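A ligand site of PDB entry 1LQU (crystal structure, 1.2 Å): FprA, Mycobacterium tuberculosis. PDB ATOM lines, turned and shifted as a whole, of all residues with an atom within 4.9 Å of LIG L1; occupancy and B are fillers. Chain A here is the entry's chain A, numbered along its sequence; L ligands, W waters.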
ATOM      1  N   ARG A 110     -22.814  23.558 -26.951  1.00  0.00           N
ATOM      2  CA  ARG A 110     -22.133  23.784 -28.189  1.00  0.00           C
ATOM      3  C   ARG A 110     -23.103  24.337 -29.229  1.00  0.00           C
ATOM      4  O   ARG A 110     -24.236  23.898 -29.350  1.00  0.00           O
ATOM      5  CB  ARG A 110     -21.509  22.506 -28.707  1.00  0.00           C
ATOM      6  CG  ARG A 110     -20.399  21.966 -27.833  1.00  0.00           C
ATOM      7  CD  ARG A 110     -19.620  20.846 -28.479  1.00  0.00           C
ATOM      8  NE  ARG A 110     -18.852  21.299 -29.626  1.00  0.00           N
ATOM      9  CZ  ARG A 110     -19.139  21.093 -30.914  1.00  0.00           C
ATOM     10  NH1 ARG A 110     -20.249  20.486 -31.293  1.00  0.00           N
ATOM     11  NH2 ARG A 110     -18.300  21.527 -31.841  1.00  0.00           N
ATOM     12  N   LEU A 112     -23.940  25.484 -33.336  1.00  0.00           N
ATOM     13  CA  LEU A 112     -23.751  25.098 -34.742  1.00  0.00           C
ATOM     14  C   LEU A 112     -22.933  26.118 -35.535  1.00  0.00           C
ATOM     15  O   LEU A 112     -22.280  25.746 -36.510  1.00  0.00           O
ATOM     16  CB  LEU A 112     -25.108  24.966 -35.425  1.00  0.00           C
ATOM     17  CG  LEU A 112     -26.025  23.889 -34.843  1.00  0.00           C
ATOM     18  CD1 LEU A 112     -27.418  24.049 -35.465  1.00  0.00           C
ATOM     19  CD2 LEU A 112     -25.470  22.500 -35.087  1.00  0.00           C
ATOM     20  N   ILE A 153     -30.764  18.279 -34.241  1.00  0.00           N
ATOM     21  CA  ILE A 153     -29.453  18.079 -34.838  1.00  0.00           C
ATOM     22  C   ILE A 153     -28.582  17.288 -33.867  1.00  0.00           C
ATOM     23  O   ILE A 153     -28.449  17.668 -32.709  1.00  0.00           O
ATOM     24  CB  ILE A 153     -28.757  19.419 -35.145  1.00  0.00           C
ATOM     25  CG1 ILE A 153     -29.660  20.366 -35.957  1.00  0.00           C
ATOM     26  CG2 ILE A 153     -27.432  19.191 -35.837  1.00  0.00           C
ATOM     27  CD1 ILE A 153     -30.123  19.845 -37.270  1.00  0.00           C
ATOM     28  N   GLY A 154     -27.974  16.233 -34.357  1.00  0.00           N
ATOM     29  CA  GLY A 154     -27.081  15.441 -33.576  1.00  0.00           C
ATOM     30  C   GLY A 154     -27.421  13.974 -33.492  1.00  0.00           C
ATOM     31  O   GLY A 154     -28.575  13.604 -33.667  1.00  0.00           O
ATOM     32  N   ASN A 155     -26.431  13.157 -33.181  1.00  0.00           N
ATOM     33  CA  ASN A 155     -26.581  11.693 -33.128  1.00  0.00           C
ATOM     34  C   ASN A 155     -26.024  11.089 -31.846  1.00  0.00           C
ATOM     35  O   ASN A 155     -25.454  10.015 -31.832  1.00  0.00           O
ATOM     36  CB  ASN A 155     -25.946  10.973 -34.334  1.00  0.00           C
ATOM     37  CG  ASN A 155     -26.806  10.885 -35.587  1.00  0.00           C
ATOM     38  OD1 ASN A 155     -26.336  10.321 -36.562  1.00  0.00           O
ATOM     39  ND2 ASN A 155     -28.014  11.455 -35.595  1.00  0.00           N
ATOM     40  N   GLY A 156     -26.238  11.800 -30.724  1.00  0.00           N
ATOM     41  CA  GLY A 156     -25.984  11.278 -29.407  1.00  0.00           C
ATOM     42  C   GLY A 156     -27.276  10.965 -28.688  1.00  0.00           C
ATOM     43  O   GLY A 156     -28.379  11.247 -29.157  1.00  0.00           O
ATOM     44  N   ASN A 157     -27.127  10.342 -27.521  1.00  0.00           N
ATOM     45  CA  ASN A 157     -28.299   9.958 -26.777  1.00  0.00           C
ATOM     46  C   ASN A 157     -29.141  11.122 -26.298  1.00  0.00           C
ATOM     47  O   ASN A 157     -30.339  10.954 -26.069  1.00  0.00           O
ATOM     48  CB  ASN A 157     -27.901   9.081 -25.603  1.00  0.00           C
ATOM     49  CG  ASN A 157     -27.454   7.697 -26.006  1.00  0.00           C
ATOM     50  OD1 ASN A 157     -27.897   7.152 -27.024  1.00  0.00           O
ATOM     51  ND2 ASN A 157     -26.615   7.105 -25.176  1.00  0.00           N
ATOM     52  N   VAL A 158     -28.566  12.310 -26.142  1.00  0.00           N
ATOM     53  CA  VAL A 158     -29.395  13.446 -25.759  1.00  0.00           C
ATOM     54  C   VAL A 158     -30.395  13.753 -26.889  1.00  0.00           C
ATOM     55  O   VAL A 158     -31.511  14.156 -26.629  1.00  0.00           O
ATOM     56  CB  VAL A 158     -28.556  14.651 -25.351  1.00  0.00           C
ATOM     57  CG1 VAL A 158     -29.457  15.856 -25.075  1.00  0.00           C
ATOM     58  CG2 VAL A 158     -27.747  14.315 -24.125  1.00  0.00           C
ATOM     59  N   ALA A 159     -29.995  13.588 -28.141  1.00  0.00           N
ATOM     60  CA  ALA A 159     -30.901  13.812 -29.248  1.00  0.00           C
ATOM     61  C   ALA A 159     -32.103  12.896 -29.142  1.00  0.00           C
ATOM     62  O   ALA A 159     -33.222  13.283 -29.453  1.00  0.00           O
ATOM     63  CB  ALA A 159     -30.202  13.592 -30.549  1.00  0.00           C
ATOM     64  N   ASP A 161     -33.298  11.574 -26.300  1.00  0.00           N
ATOM     65  CA  ASP A 161     -34.143  12.062 -25.200  1.00  0.00           C
ATOM     66  C   ASP A 161     -35.040  13.207 -25.705  1.00  0.00           C
ATOM     67  O   ASP A 161     -36.228  13.234 -25.414  1.00  0.00           O
ATOM     68  CB  ASP A 161     -33.292  12.591 -24.057  1.00  0.00           C
ATOM     69  CG  ASP A 161     -32.688  11.537 -23.185  1.00  0.00           C
ATOM     70  OD1 ASP A 161     -32.912  10.332 -23.387  1.00  0.00           O
ATOM     71  OD2 ASP A 161     -31.967  11.893 -22.225  1.00  0.00           O
ATOM     72  N   ARG A 199     -24.745  14.330 -38.945  1.00  0.00           N
ATOM     73  CA  ARG A 199     -23.823  14.772 -39.973  1.00  0.00           C
ATOM     74  C   ARG A 199     -22.997  13.663 -40.598  1.00  0.00           C
ATOM     75  O   ARG A 199     -22.700  13.716 -41.791  1.00  0.00           O
ATOM     76  CB  ARG A 199     -22.932  15.917 -39.456  1.00  0.00           C
ATOM     77  CG  ARG A 199     -21.975  15.570 -38.334  1.00  0.00           C
ATOM     78  CD  ARG A 199     -21.028  16.708 -38.072  1.00  0.00           C
ATOM     79  NE  ARG A 199     -20.233  16.425 -36.904  1.00  0.00           N
ATOM     80  CZ  ARG A 199     -19.393  17.299 -36.360  1.00  0.00           C
ATOM     81  NH1 ARG A 199     -19.297  18.499 -36.901  1.00  0.00           N
ATOM     82  NH2 ARG A 199     -18.717  16.985 -35.279  1.00  0.00           N
ATOM     83  N   ARG A 200     -22.602  12.692 -39.790  1.00  0.00           N
ATOM     84  CA  ARG A 200     -21.917  11.516 -40.303  1.00  0.00           C
ATOM     85  C   ARG A 200     -22.933  10.396 -40.487  1.00  0.00           C
ATOM     86  O   ARG A 200     -24.118  10.659 -40.597  1.00  0.00           O
ATOM     87  CB  ARG A 200     -20.727  11.154 -39.445  1.00  0.00           C
ATOM     88  CG  ARG A 200     -19.665  12.273 -39.430  1.00  0.00           C
ATOM     89  CD  ARG A 200     -18.328  11.876 -38.820  1.00  0.00           C
ATOM     90  NE  ARG A 200     -18.464  11.634 -37.395  1.00  0.00           N
ATOM     91  CZ  ARG A 200     -17.641  10.914 -36.674  1.00  0.00           C
ATOM     92  NH1 ARG A 200     -16.593  10.312 -37.230  1.00  0.00           N
ATOM     93  NH2 ARG A 200     -17.869  10.755 -35.394  1.00  0.00           N
ATOM     94  N   GLN A 204     -21.032   5.980 -37.355  1.00  0.00           N
ATOM     95  CA  GLN A 204     -20.395   7.001 -36.543  1.00  0.00           C
ATOM     96  C   GLN A 204     -21.319   7.537 -35.449  1.00  0.00           C
ATOM     97  O   GLN A 204     -20.938   8.432 -34.704  1.00  0.00           O
ATOM     98  CB  GLN A 204     -19.917   8.164 -37.404  1.00  0.00           C
ATOM     99  CG  GLN A 204     -18.797   7.815 -38.343  1.00  0.00           C
ATOM    100  CD  GLN A 204     -19.239   7.062 -39.590  1.00  0.00           C
ATOM    101  OE1 GLN A 204     -20.287   7.346 -40.170  1.00  0.00           O
ATOM    102  NE2 GLN A 204     -18.421   6.081 -40.004  1.00  0.00           N
ATOM    103  N   ALA A 206     -23.274   8.242 -32.098  1.00  0.00           N
ATOM    104  CA  ALA A 206     -22.875   8.135 -30.685  1.00  0.00           C
ATOM    105  C   ALA A 206     -23.994   7.541 -29.819  1.00  0.00           C
ATOM    106  O   ALA A 206     -23.825   7.373 -28.627  1.00  0.00           O
ATOM    107  CB  ALA A 206     -22.471   9.488 -30.182  1.00  0.00           C
ATOM    108  N   THR A 208     -26.362   4.758 -28.074  1.00  0.00           N
ATOM    109  CA  THR A 208     -26.134   3.402 -27.577  1.00  0.00           C
ATOM    110  C   THR A 208     -27.398   2.549 -27.769  1.00  0.00           C
ATOM    111  O   THR A 208     -28.467   3.060 -28.078  1.00  0.00           O
ATOM    112  CB  THR A 208     -25.586   3.391 -26.144  1.00  0.00           C
ATOM    113  OG1 THR A 208     -26.388   4.221 -25.309  1.00  0.00           O
ATOM    114  CG2 THR A 208     -24.193   3.989 -26.104  1.00  0.00           C
ATOM    115  N   GLU A 211     -30.941   2.549 -25.848  1.00  0.00           N
ATOM    116  CA  GLU A 211     -31.563   3.817 -26.104  1.00  0.00           C
ATOM    117  C   GLU A 211     -32.258   3.829 -27.473  1.00  0.00           C
ATOM    118  O   GLU A 211     -33.317   4.412 -27.652  1.00  0.00           O
ATOM    119  CB  GLU A 211     -30.520   4.919 -25.950  1.00  0.00           C
ATOM    120  CG  GLU A 211     -30.150   5.124 -24.489  1.00  0.00           C
ATOM    121  CD  GLU A 211     -29.447   3.957 -23.789  1.00  0.00           C
ATOM    122  OE1 GLU A 211     -28.594   3.260 -24.389  1.00  0.00           O
ATOM    123  OE2 GLU A 211     -29.713   3.775 -22.576  1.00  0.00           O
ATOM    124  N   PRO A 275     -27.027  20.844 -40.923  1.00  0.00           N
ATOM    125  CA  PRO A 275     -27.804  22.078 -41.013  1.00  0.00           C
ATOM    126  C   PRO A 275     -26.891  23.187 -41.546  1.00  0.00           C
ATOM    127  O   PRO A 275     -25.806  23.420 -41.048  1.00  0.00           O
ATOM    128  CB  PRO A 275     -28.213  22.328 -39.564  1.00  0.00           C
ATOM    129  CG  PRO A 275     -27.096  21.764 -38.734  1.00  0.00           C
ATOM    130  CD  PRO A 275     -26.628  20.530 -39.530  1.00  0.00           C
ATOM    131  N   SER A 321     -28.607  19.345 -30.570  1.00  0.00           N
ATOM    132  CA  SER A 321     -28.059  18.432 -29.557  1.00  0.00           C
ATOM    133  C   SER A 321     -26.686  18.003 -30.012  1.00  0.00           C
ATOM    134  O   SER A 321     -26.437  16.827 -30.296  1.00  0.00           O
ATOM    135  CB  SER A 321     -29.007  17.249 -29.326  1.00  0.00           C
ATOM    136  OG  SER A 321     -28.583  16.524 -28.201  1.00  0.00           O
ATOM    137  N   VAL A 322     -25.792  18.974 -30.065  1.00  0.00           N
ATOM    138  CA  VAL A 322     -24.457  18.779 -30.577  1.00  0.00           C
ATOM    139  C   VAL A 322     -23.418  18.835 -29.494  1.00  0.00           C
ATOM    140  O   VAL A 322     -22.227  19.038 -29.745  1.00  0.00           O
ATOM    141  CB  VAL A 322     -24.150  19.654 -31.797  1.00  0.00           C
ATOM    142  CG1 VAL A 322     -25.153  19.317 -32.902  1.00  0.00           C
ATOM    143  CG2 VAL A 322     -24.167  21.146 -31.511  1.00  0.00           C
ATOM    144  N   GLY A 323     -23.868  18.590 -28.268  1.00  0.00           N
ATOM    145  CA  GLY A 323     -22.995  18.521 -27.107  1.00  0.00           C
ATOM    146  C   GLY A 323     -23.233  19.609 -26.110  1.00  0.00           C
ATOM    147  O   GLY A 323     -23.582  20.736 -26.463  1.00  0.00           O
ATOM    148  N   TYR A 324     -23.018  19.257 -24.858  1.00  0.00           N
ATOM    149  CA  TYR A 324     -22.932  20.218 -23.784  1.00  0.00           C
ATOM    150  C   TYR A 324     -21.530  20.860 -23.823  1.00  0.00           C
ATOM    151  O   TYR A 324     -20.688  20.422 -24.601  1.00  0.00           O
ATOM    152  CB  TYR A 324     -23.195  19.540 -22.440  1.00  0.00           C
ATOM    153  CG  TYR A 324     -24.673  19.329 -22.105  1.00  0.00           C
ATOM    154  CD1 TYR A 324     -25.539  18.691 -22.979  1.00  0.00           C
ATOM    155  CD2 TYR A 324     -25.180  19.770 -20.898  1.00  0.00           C
ATOM    156  CE1 TYR A 324     -26.872  18.560 -22.668  1.00  0.00           C
ATOM    157  CE2 TYR A 324     -26.519  19.603 -20.591  1.00  0.00           C
ATOM    158  CZ  TYR A 324     -27.367  19.012 -21.483  1.00  0.00           C
ATOM    159  OH  TYR A 324     -28.714  18.867 -21.197  1.00  0.00           O
ATOM    160  N   TRP A 359     -17.238  15.907 -16.060  1.00  0.00           N
ATOM    161  CA  TRP A 359     -17.273  16.482 -17.384  1.00  0.00           C
ATOM    162  C   TRP A 359     -16.437  17.735 -17.540  1.00  0.00           C
ATOM    163  O   TRP A 359     -15.985  18.018 -18.623  1.00  0.00           O
ATOM    164  CB  TRP A 359     -18.716  16.709 -17.795  1.00  0.00           C
ATOM    165  CG  TRP A 359     -19.449  15.475 -18.171  1.00  0.00           C
ATOM    166  CD1 TRP A 359     -19.008  14.178 -18.033  1.00  0.00           C
ATOM    167  CD2 TRP A 359     -20.703  15.392 -18.863  1.00  0.00           C
ATOM    168  NE1 TRP A 359     -19.926  13.317 -18.575  1.00  0.00           N
ATOM    169  CE2 TRP A 359     -20.942  14.049 -19.127  1.00  0.00           C
ATOM    170  CE3 TRP A 359     -21.596  16.346 -19.342  1.00  0.00           C
ATOM    171  CZ2 TRP A 359     -22.056  13.634 -19.830  1.00  0.00           C
ATOM    172  CZ3 TRP A 359     -22.701  15.924 -20.027  1.00  0.00           C
ATOM    173  CH2 TRP A 359     -22.926  14.596 -20.266  1.00  0.00           C
ATOM    174  N   PRO A 364     -17.689  16.490 -22.078  1.00  0.00           N
ATOM    175  CA  PRO A 364     -19.065  16.092 -21.770  1.00  0.00           C
ATOM    176  C   PRO A 364     -19.494  14.806 -22.374  1.00  0.00           C
ATOM    177  O   PRO A 364     -20.485  14.790 -23.123  1.00  0.00           O
ATOM    178  CB  PRO A 364     -19.870  17.268 -22.343  1.00  0.00           C
ATOM    179  CG  PRO A 364     -19.079  17.637 -23.556  1.00  0.00           C
ATOM    180  CD  PRO A 364     -17.649  17.556 -23.093  1.00  0.00           C
ATOM    181  N   THR A 365     -18.821  13.725 -22.022  1.00  0.00           N
ATOM    182  CA  THR A 365     -19.232  12.411 -22.482  1.00  0.00           C
ATOM    183  C   THR A 365     -19.106  11.389 -21.358  1.00  0.00           C
ATOM    184  O   THR A 365     -18.277  11.500 -20.443  1.00  0.00           O
ATOM    185  CB  THR A 365     -18.527  11.944 -23.741  1.00  0.00           C
ATOM    186  OG1 THR A 365     -17.158  11.857 -23.453  1.00  0.00           O
ATOM    187  CG2 THR A 365     -18.702  12.896 -24.917  1.00  0.00           C
ATOM    188  N   GLY A 366     -19.985  10.422 -21.427  1.00  0.00           N
ATOM    189  CA  GLY A 366     -19.991   9.274 -20.542  1.00  0.00           C
ATOM    190  C   GLY A 366     -21.229   9.200 -19.688  1.00  0.00           C
ATOM    191  O   GLY A 366     -21.735  10.224 -19.213  1.00  0.00           O
ATOM    192  N   VAL A 367     -21.683   7.978 -19.467  1.00  0.00           N
ATOM    193  CA  VAL A 367     -22.763   7.683 -18.549  1.00  0.00           C
ATOM    194  C   VAL A 367     -22.322   8.001 -17.106  1.00  0.00           C
ATOM    195  O   VAL A 367     -21.155   8.244 -16.797  1.00  0.00           O
ATOM    196  CB  VAL A 367     -23.220   6.227 -18.643  1.00  0.00           C
ATOM    197  CG1 VAL A 367     -23.838   5.949 -19.999  1.00  0.00           C
ATOM    198  CG2 VAL A 367     -22.099   5.227 -18.367  1.00  0.00           C
HETATM  199  P1  LIG L   1     -22.565  12.952 -27.711  1.00  0.00           P
HETATM  200  O1  LIG L   1     -22.944  11.575 -27.382  1.00  0.00           O
HETATM  201  O2  LIG L   1     -21.128  13.308 -27.730  1.00  0.00           O
HETATM  202  O3  LIG L   1     -23.224  13.286 -29.124  1.00  0.00           O
HETATM  203  C1  LIG L   1     -22.979  14.528 -29.715  1.00  0.00           C
HETATM  204  C2  LIG L   1     -23.481  14.492 -31.140  1.00  0.00           C
HETATM  205  O4  LIG L   1     -23.367  15.808 -31.735  1.00  0.00           O
HETATM  206  C3  LIG L   1     -22.679  13.559 -32.037  1.00  0.00           C
HETATM  207  O5  LIG L   1     -23.592  12.830 -32.851  1.00  0.00           O
HETATM  208  C4  LIG L   1     -21.853  14.525 -32.890  1.00  0.00           C
HETATM  209  O6  LIG L   1     -21.512  14.030 -34.159  1.00  0.00           O
HETATM  210  C5  LIG L   1     -22.840  15.631 -33.024  1.00  0.00           C
HETATM  211  N1  LIG L   1     -22.319  16.902 -33.492  1.00  0.00           N
HETATM  212  C6  LIG L   1     -21.305  17.658 -32.919  1.00  0.00           C
HETATM  213  N2  LIG L   1     -21.136  18.779 -33.603  1.00  0.00           N
HETATM  214  C7  LIG L   1     -22.038  18.773 -34.634  1.00  0.00           C
HETATM  215  C8  LIG L   1     -22.332  19.667 -35.639  1.00  0.00           C
HETATM  216  N3  LIG L   1     -21.775  20.888 -35.755  1.00  0.00           N
HETATM  217  N4  LIG L   1     -23.332  19.337 -36.528  1.00  0.00           N
HETATM  218  C9  LIG L   1     -24.000  18.147 -36.392  1.00  0.00           C
HETATM  219  N5  LIG L   1     -23.740  17.232 -35.424  1.00  0.00           N
HETATM  220  C10 LIG L   1     -22.776  17.591 -34.565  1.00  0.00           C
HETATM  221  O7  LIG L   1     -23.263  14.018 -26.737  1.00  0.00           O
HETATM  222  P2  LIG L   1     -24.710  14.121 -26.032  1.00  0.00           P
HETATM  223  O8  LIG L   1     -25.766  13.528 -26.884  1.00  0.00           O
HETATM  224  O9  LIG L   1     -24.779  15.519 -25.610  1.00  0.00           O
HETATM  225  O10 LIG L   1     -24.569  13.133 -24.804  1.00  0.00           O
HETATM  226  C11 LIG L   1     -23.638  13.450 -23.764  1.00  0.00           C
HETATM  227  C12 LIG L   1     -23.210  12.180 -23.024  1.00  0.00           C
HETATM  228  O11 LIG L   1     -24.248  11.768 -22.110  1.00  0.00           O
HETATM  229  C13 LIG L   1     -22.953  11.030 -23.973  1.00  0.00           C
HETATM  230  O12 LIG L   1     -21.873  10.259 -23.504  1.00  0.00           O
HETATM  231  C14 LIG L   1     -24.250  10.243 -23.859  1.00  0.00           C
HETATM  232  O13 LIG L   1     -24.245   8.908 -24.264  1.00  0.00           O
HETATM  233  C15 LIG L   1     -24.682  10.464 -22.445  1.00  0.00           C
HETATM  234  N6  LIG L   1     -25.989  10.162 -22.008  1.00  0.00           N
HETATM  235  C16 LIG L   1     -26.341   8.870 -21.752  1.00  0.00           C
HETATM  236  C17 LIG L   1     -27.675   8.490 -21.877  1.00  0.00           C
HETATM  237  C18 LIG L   1     -27.932   7.098 -21.615  1.00  0.00           C
HETATM  238  O14 LIG L   1     -26.961   6.250 -21.374  1.00  0.00           O
HETATM  239  N7  LIG L   1     -29.203   6.704 -21.662  1.00  0.00           N
HETATM  240  C19 LIG L   1     -28.734   9.448 -22.178  1.00  0.00           C
HETATM  241  C20 LIG L   1     -28.267  10.839 -22.515  1.00  0.00           C
HETATM  242  C21 LIG L   1     -26.919  11.122 -22.451  1.00  0.00           C
HETATM  243  P3  LIG L   1     -20.015  13.575 -34.528  1.00  0.00           P
HETATM  244  O15 LIG L   1     -20.017  13.595 -36.034  1.00  0.00           O
HETATM  245  O16 LIG L   1     -19.819  12.206 -33.941  1.00  0.00           O
HETATM  246  O17 LIG L   1     -19.068  14.588 -33.901  1.00  0.00           O
HETATM  247  P1  LG2 L   2     -23.135  17.373 -13.455  1.00  0.00           P
HETATM  248  O1  LG2 L   2     -23.509  18.326 -14.515  1.00  0.00           O
HETATM  249  O2  LG2 L   2     -23.990  16.192 -13.202  1.00  0.00           O
HETATM  250  O3  LG2 L   2     -23.005  18.146 -12.071  1.00  0.00           O
HETATM  251  C1  LG2 L   2     -22.390  19.435 -12.051  1.00  0.00           C
HETATM  252  C2  LG2 L   2     -22.927  20.158 -10.810  1.00  0.00           C
HETATM  253  O4  LG2 L   2     -22.114  21.317 -10.589  1.00  0.00           O
HETATM  254  C3  LG2 L   2     -24.374  20.653 -10.928  1.00  0.00           C
HETATM  255  O5  LG2 L   2     -25.165  20.300  -9.804  1.00  0.00           O
HETATM  256  C4  LG2 L   2     -24.212  22.158 -11.094  1.00  0.00           C
HETATM  257  O6  LG2 L   2     -25.316  22.953 -10.705  1.00  0.00           O
HETATM  258  C5  LG2 L   2     -22.951  22.414 -10.257  1.00  0.00           C
HETATM  259  N1  LG2 L   2     -22.239  23.644 -10.594  1.00  0.00           N
HETATM  260  C6  LG2 L   2     -21.864  24.064 -11.848  1.00  0.00           C
HETATM  261  N2  LG2 L   2     -21.205  25.220 -11.760  1.00  0.00           N
HETATM  262  C7  LG2 L   2     -21.182  25.571 -10.421  1.00  0.00           C
HETATM  263  C8  LG2 L   2     -20.650  26.674  -9.779  1.00  0.00           C
HETATM  264  N3  LG2 L   2     -19.963  27.645 -10.403  1.00  0.00           N
HETATM  265  N4  LG2 L   2     -20.767  26.711  -8.420  1.00  0.00           N
HETATM  266  C9  LG2 L   2     -21.396  25.701  -7.786  1.00  0.00           C
HETATM  267  N5  LG2 L   2     -21.950  24.617  -8.368  1.00  0.00           N
HETATM  268  C10 LG2 L   2     -21.808  24.573  -9.700  1.00  0.00           C
HETATM  269  N6  LG2 L   2     -26.056   9.126 -17.822  1.00  0.00           N
HETATM  270  C11 LG2 L   2     -26.560   7.893 -17.606  1.00  0.00           C
HETATM  271  O7  LG2 L   2     -25.868   7.007 -17.091  1.00  0.00           O
HETATM  272  N7  LG2 L   2     -27.867   7.637 -17.959  1.00  0.00           N
HETATM  273  C12 LG2 L   2     -28.705   8.599 -18.484  1.00  0.00           C
HETATM  274  O8  LG2 L   2     -29.900   8.311 -18.752  1.00  0.00           O
HETATM  275  C13 LG2 L   2     -28.179   9.876 -18.649  1.00  0.00           C
HETATM  276  N8  LG2 L   2     -28.977  10.903 -19.094  1.00  0.00           N
HETATM  277  C14 LG2 L   2     -28.386  12.132 -19.381  1.00  0.00           C
HETATM  278  C15 LG2 L   2     -29.123  13.123 -19.979  1.00  0.00           C
HETATM  279  C16 LG2 L   2     -28.601  14.344 -20.350  1.00  0.00           C
HETATM  280  C17 LG2 L   2     -29.484  15.410 -20.958  1.00  0.00           C
HETATM  281  C18 LG2 L   2     -27.238  14.552 -20.115  1.00  0.00           C
HETATM  282  C19 LG2 L   2     -26.595  15.833 -20.505  1.00  0.00           C
HETATM  283  C20 LG2 L   2     -26.469  13.558 -19.519  1.00  0.00           C
HETATM  284  C21 LG2 L   2     -27.022  12.338 -19.163  1.00  0.00           C
HETATM  285  N9  LG2 L   2     -26.261  11.316 -18.578  1.00  0.00           N
HETATM  286  C22 LG2 L   2     -26.845  10.113 -18.326  1.00  0.00           C
HETATM  287  C23 LG2 L   2     -24.815  11.517 -18.251  1.00  0.00           C
HETATM  288  C24 LG2 L   2     -24.649  12.082 -16.841  1.00  0.00           C
HETATM  289  O9  LG2 L   2     -25.578  13.103 -16.682  1.00  0.00           O
HETATM  290  C25 LG2 L   2     -23.201  12.573 -16.635  1.00  0.00           C
HETATM  291  O10 LG2 L   2     -22.272  11.516 -16.785  1.00  0.00           O
HETATM  292  C26 LG2 L   2     -22.926  13.163 -15.261  1.00  0.00           C
HETATM  293  O11 LG2 L   2     -24.047  13.834 -14.707  1.00  0.00           O
HETATM  294  C27 LG2 L   2     -21.737  14.111 -15.312  1.00  0.00           C
HETATM  295  O12 LG2 L   2     -21.447  14.414 -13.956  1.00  0.00           O
HETATM  296  P2  LG2 L   2     -20.673  15.708 -13.475  1.00  0.00           P
HETATM  297  O13 LG2 L   2     -20.560  15.549 -12.010  1.00  0.00           O
HETATM  298  O14 LG2 L   2     -19.427  15.979 -14.249  1.00  0.00           O
HETATM  299  O15 LG2 L   2     -21.623  16.953 -13.825  1.00  0.00           O
HETATM  300  O   HOH W   1     -26.977  14.357 -29.168  1.00  0.00           O
HETATM  301  O   HOH W   2     -22.218  23.198 -37.544  1.00  0.00           O
HETATM  302  O   HOH W   3     -22.789   6.651 -23.463  1.00  0.00           O
HETATM  303  O   HOH W   4     -22.315  16.532 -24.610  1.00  0.00           O
HETATM  304  O   HOH W   5     -24.448   9.437 -26.880  1.00  0.00           O
HETATM  305  O   HOH W   6     -22.183  10.862 -33.949  1.00  0.00           O
HETATM  306  O   HOH W   7     -26.224  17.631 -26.760  1.00  0.00           O
HETATM  307  O   HOH W   8     -24.606  14.539 -35.989  1.00  0.00           O
HETATM  308  O   HOH W   9     -18.977  11.341 -31.656  1.00  0.00           O
HETATM  309  O   HOH W  10     -23.038  19.944 -39.216  1.00  0.00           O
HETATM  310  O   HOH W  11     -31.744   7.931 -22.539  1.00  0.00           O
HETATM  311  O   HOH W  12     -25.099   5.096 -22.947  1.00  0.00           O
HETATM  312  O   HOH W  13     -18.599  15.271 -31.346  1.00  0.00           O
HETATM  313  O   HOH W  14     -16.407  14.092 -33.760  1.00  0.00           O
HETATM  314  O   HOH W  15     -19.278  13.284 -29.647  1.00  0.00           O
HETATM  315  O   HOH W  16     -20.441  15.752 -26.747  1.00  0.00           O
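The indole nitrogen (NE1) of Trp 359 sits at hydrogen-bond distance from an oxygen (O10) of LG2 L2 (3.5 Å).
The backbone NH of Trp 359 lies within hydrogen-bond range of an oxygen (O14) of LG2 L2.
The guanidinium group of Arg 110 lies within hydrogen-bond range of a nitrogen (N2) of LIG L1 (3.0 Å).
NH2 of Arg 199 lies within salt-bridge range of O17 of LIG L1.
N of Gly 366 lies within hydrogen-bond range of O12 of LIG L1 (2.8 Å).
NH2 of Arg 200 lies within salt-bridge range of O16 of LIG L1.
An oxygen (O10) of LG2 L2 sits at hydrogen-bond distance from the backbone carbonyl oxygen (O) of Gly 366, 2.8 Å away.
O5 of LIG L1 sits at hydrogen-bond distance from N of Asn 155 (2.9 Å).
N of Val 158 lies within hydrogen-bond range of O8 of LIG L1 (3.1 Å).
The side-chain amide nitrogen (ND2) of Asn 157 lies within hydrogen-bond range of an oxygen (O13) of LIG L1 (3.1 Å).
O of Val 367 lies within hydrogen-bond range of O10 of LG2 L2 (3.5 Å).
The side-chain carboxylate (OE2) of Glu 211 is in hydrogen-bond range of a nitrogen (N7) of LIG L1, at 3.1 Å.
A nitrogen (N7) of LIG L1 lies within hydrogen-bond range of an oxygen (O8) of LG2 L2, at 3.4 Å.
N of Ala 159 sits at hydrogen-bond distance from OG of Ser 321, 3.3 Å away.
O of Gly 323 lies within hydrogen-bond range of N of Arg 110.
The side-chain carboxylate of Glu 211 is in hydrogen-bond range of the side-chain hydroxyl of Thr 208 (2.6 Å).
The guanidinium group of Arg 110 is in hydrogen-bond range of the backbone carbonyl oxygen of Val 322 (2.9 Å).
The backbone carbonyl oxygen (O) of Asn 155 lies within hydrogen-bond range of the backbone NH (N) of Ala 206.
The backbone NH (N) of Ser 321 is in hydrogen-bond range of the backbone carbonyl oxygen (O) of Ile 153.
O of Thr 365 lies within hydrogen-bond range of NE1 of Trp 359 (3.1 Å).
The side-chain amide nitrogen (ND2) of Asn 157 sits at hydrogen-bond distance from the side-chain hydroxyl (OG1) of Thr 208, at 2.9 Å.
Merely in contact with LIG L1: Val 322, Gly 156, Val 367, Pro 364, Ala 206, Ser 321, Thr 365, Trp 359, Ile 153, Gly 323 and Asp 161.
Hydrophobic or aromatic side chains that line LIG L1: Ile 153, Val 158, Ala 206, Val 322, Trp 359 and Val 367.
Within 4 Å of LIG L1: Arg 110, Ile 153, Asn 155, Gly 156, Asn 157, Val 158, Asp 161, Arg 199, Arg 200, Ala 206, Glu 211, Ser 321, Val 322, Gly 323, Trp 359, Pro 364, Thr 365, Gly 366 and Val 367.
Water W6 lies within hydrogen-bond range of an oxygen (O5) of LIG L1 (2.7 Å), the backbone carbonyl oxygen (O) of Gln 204 (2.8 Å) and the backbone NH (N) of Ala 206 (3.4 Å).
Water W12 lies within hydrogen-bond range of an oxygen (O14) of LIG L1 (2.7 Å), the side-chain hydroxyl (OG1) of Thr 208 (2.8 Å) and the side-chain amide nitrogen (ND2) of Asn 157 (3.4 Å).
Water W7 lies within hydrogen-bond range of O9 of LIG L1 (2.8 Å), N of Gly 323 (3.0 Å) and OG of Ser 321 (3.0 Å).
Water W4 lies within hydrogen-bond range of the backbone NH (N) of Tyr 324, an oxygen (O9) of LIG L1 and the backbone carbonyl oxygen (O) of Pro 364.
Water W11 bridges OD1 of Asp 161 and N7 of LIG L1.
Water W2 lies within hydrogen-bond range of the backbone carbonyl oxygen of Leu 112 (2.8 Å) and a nitrogen (N3) of LIG L1 (3.0 Å).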
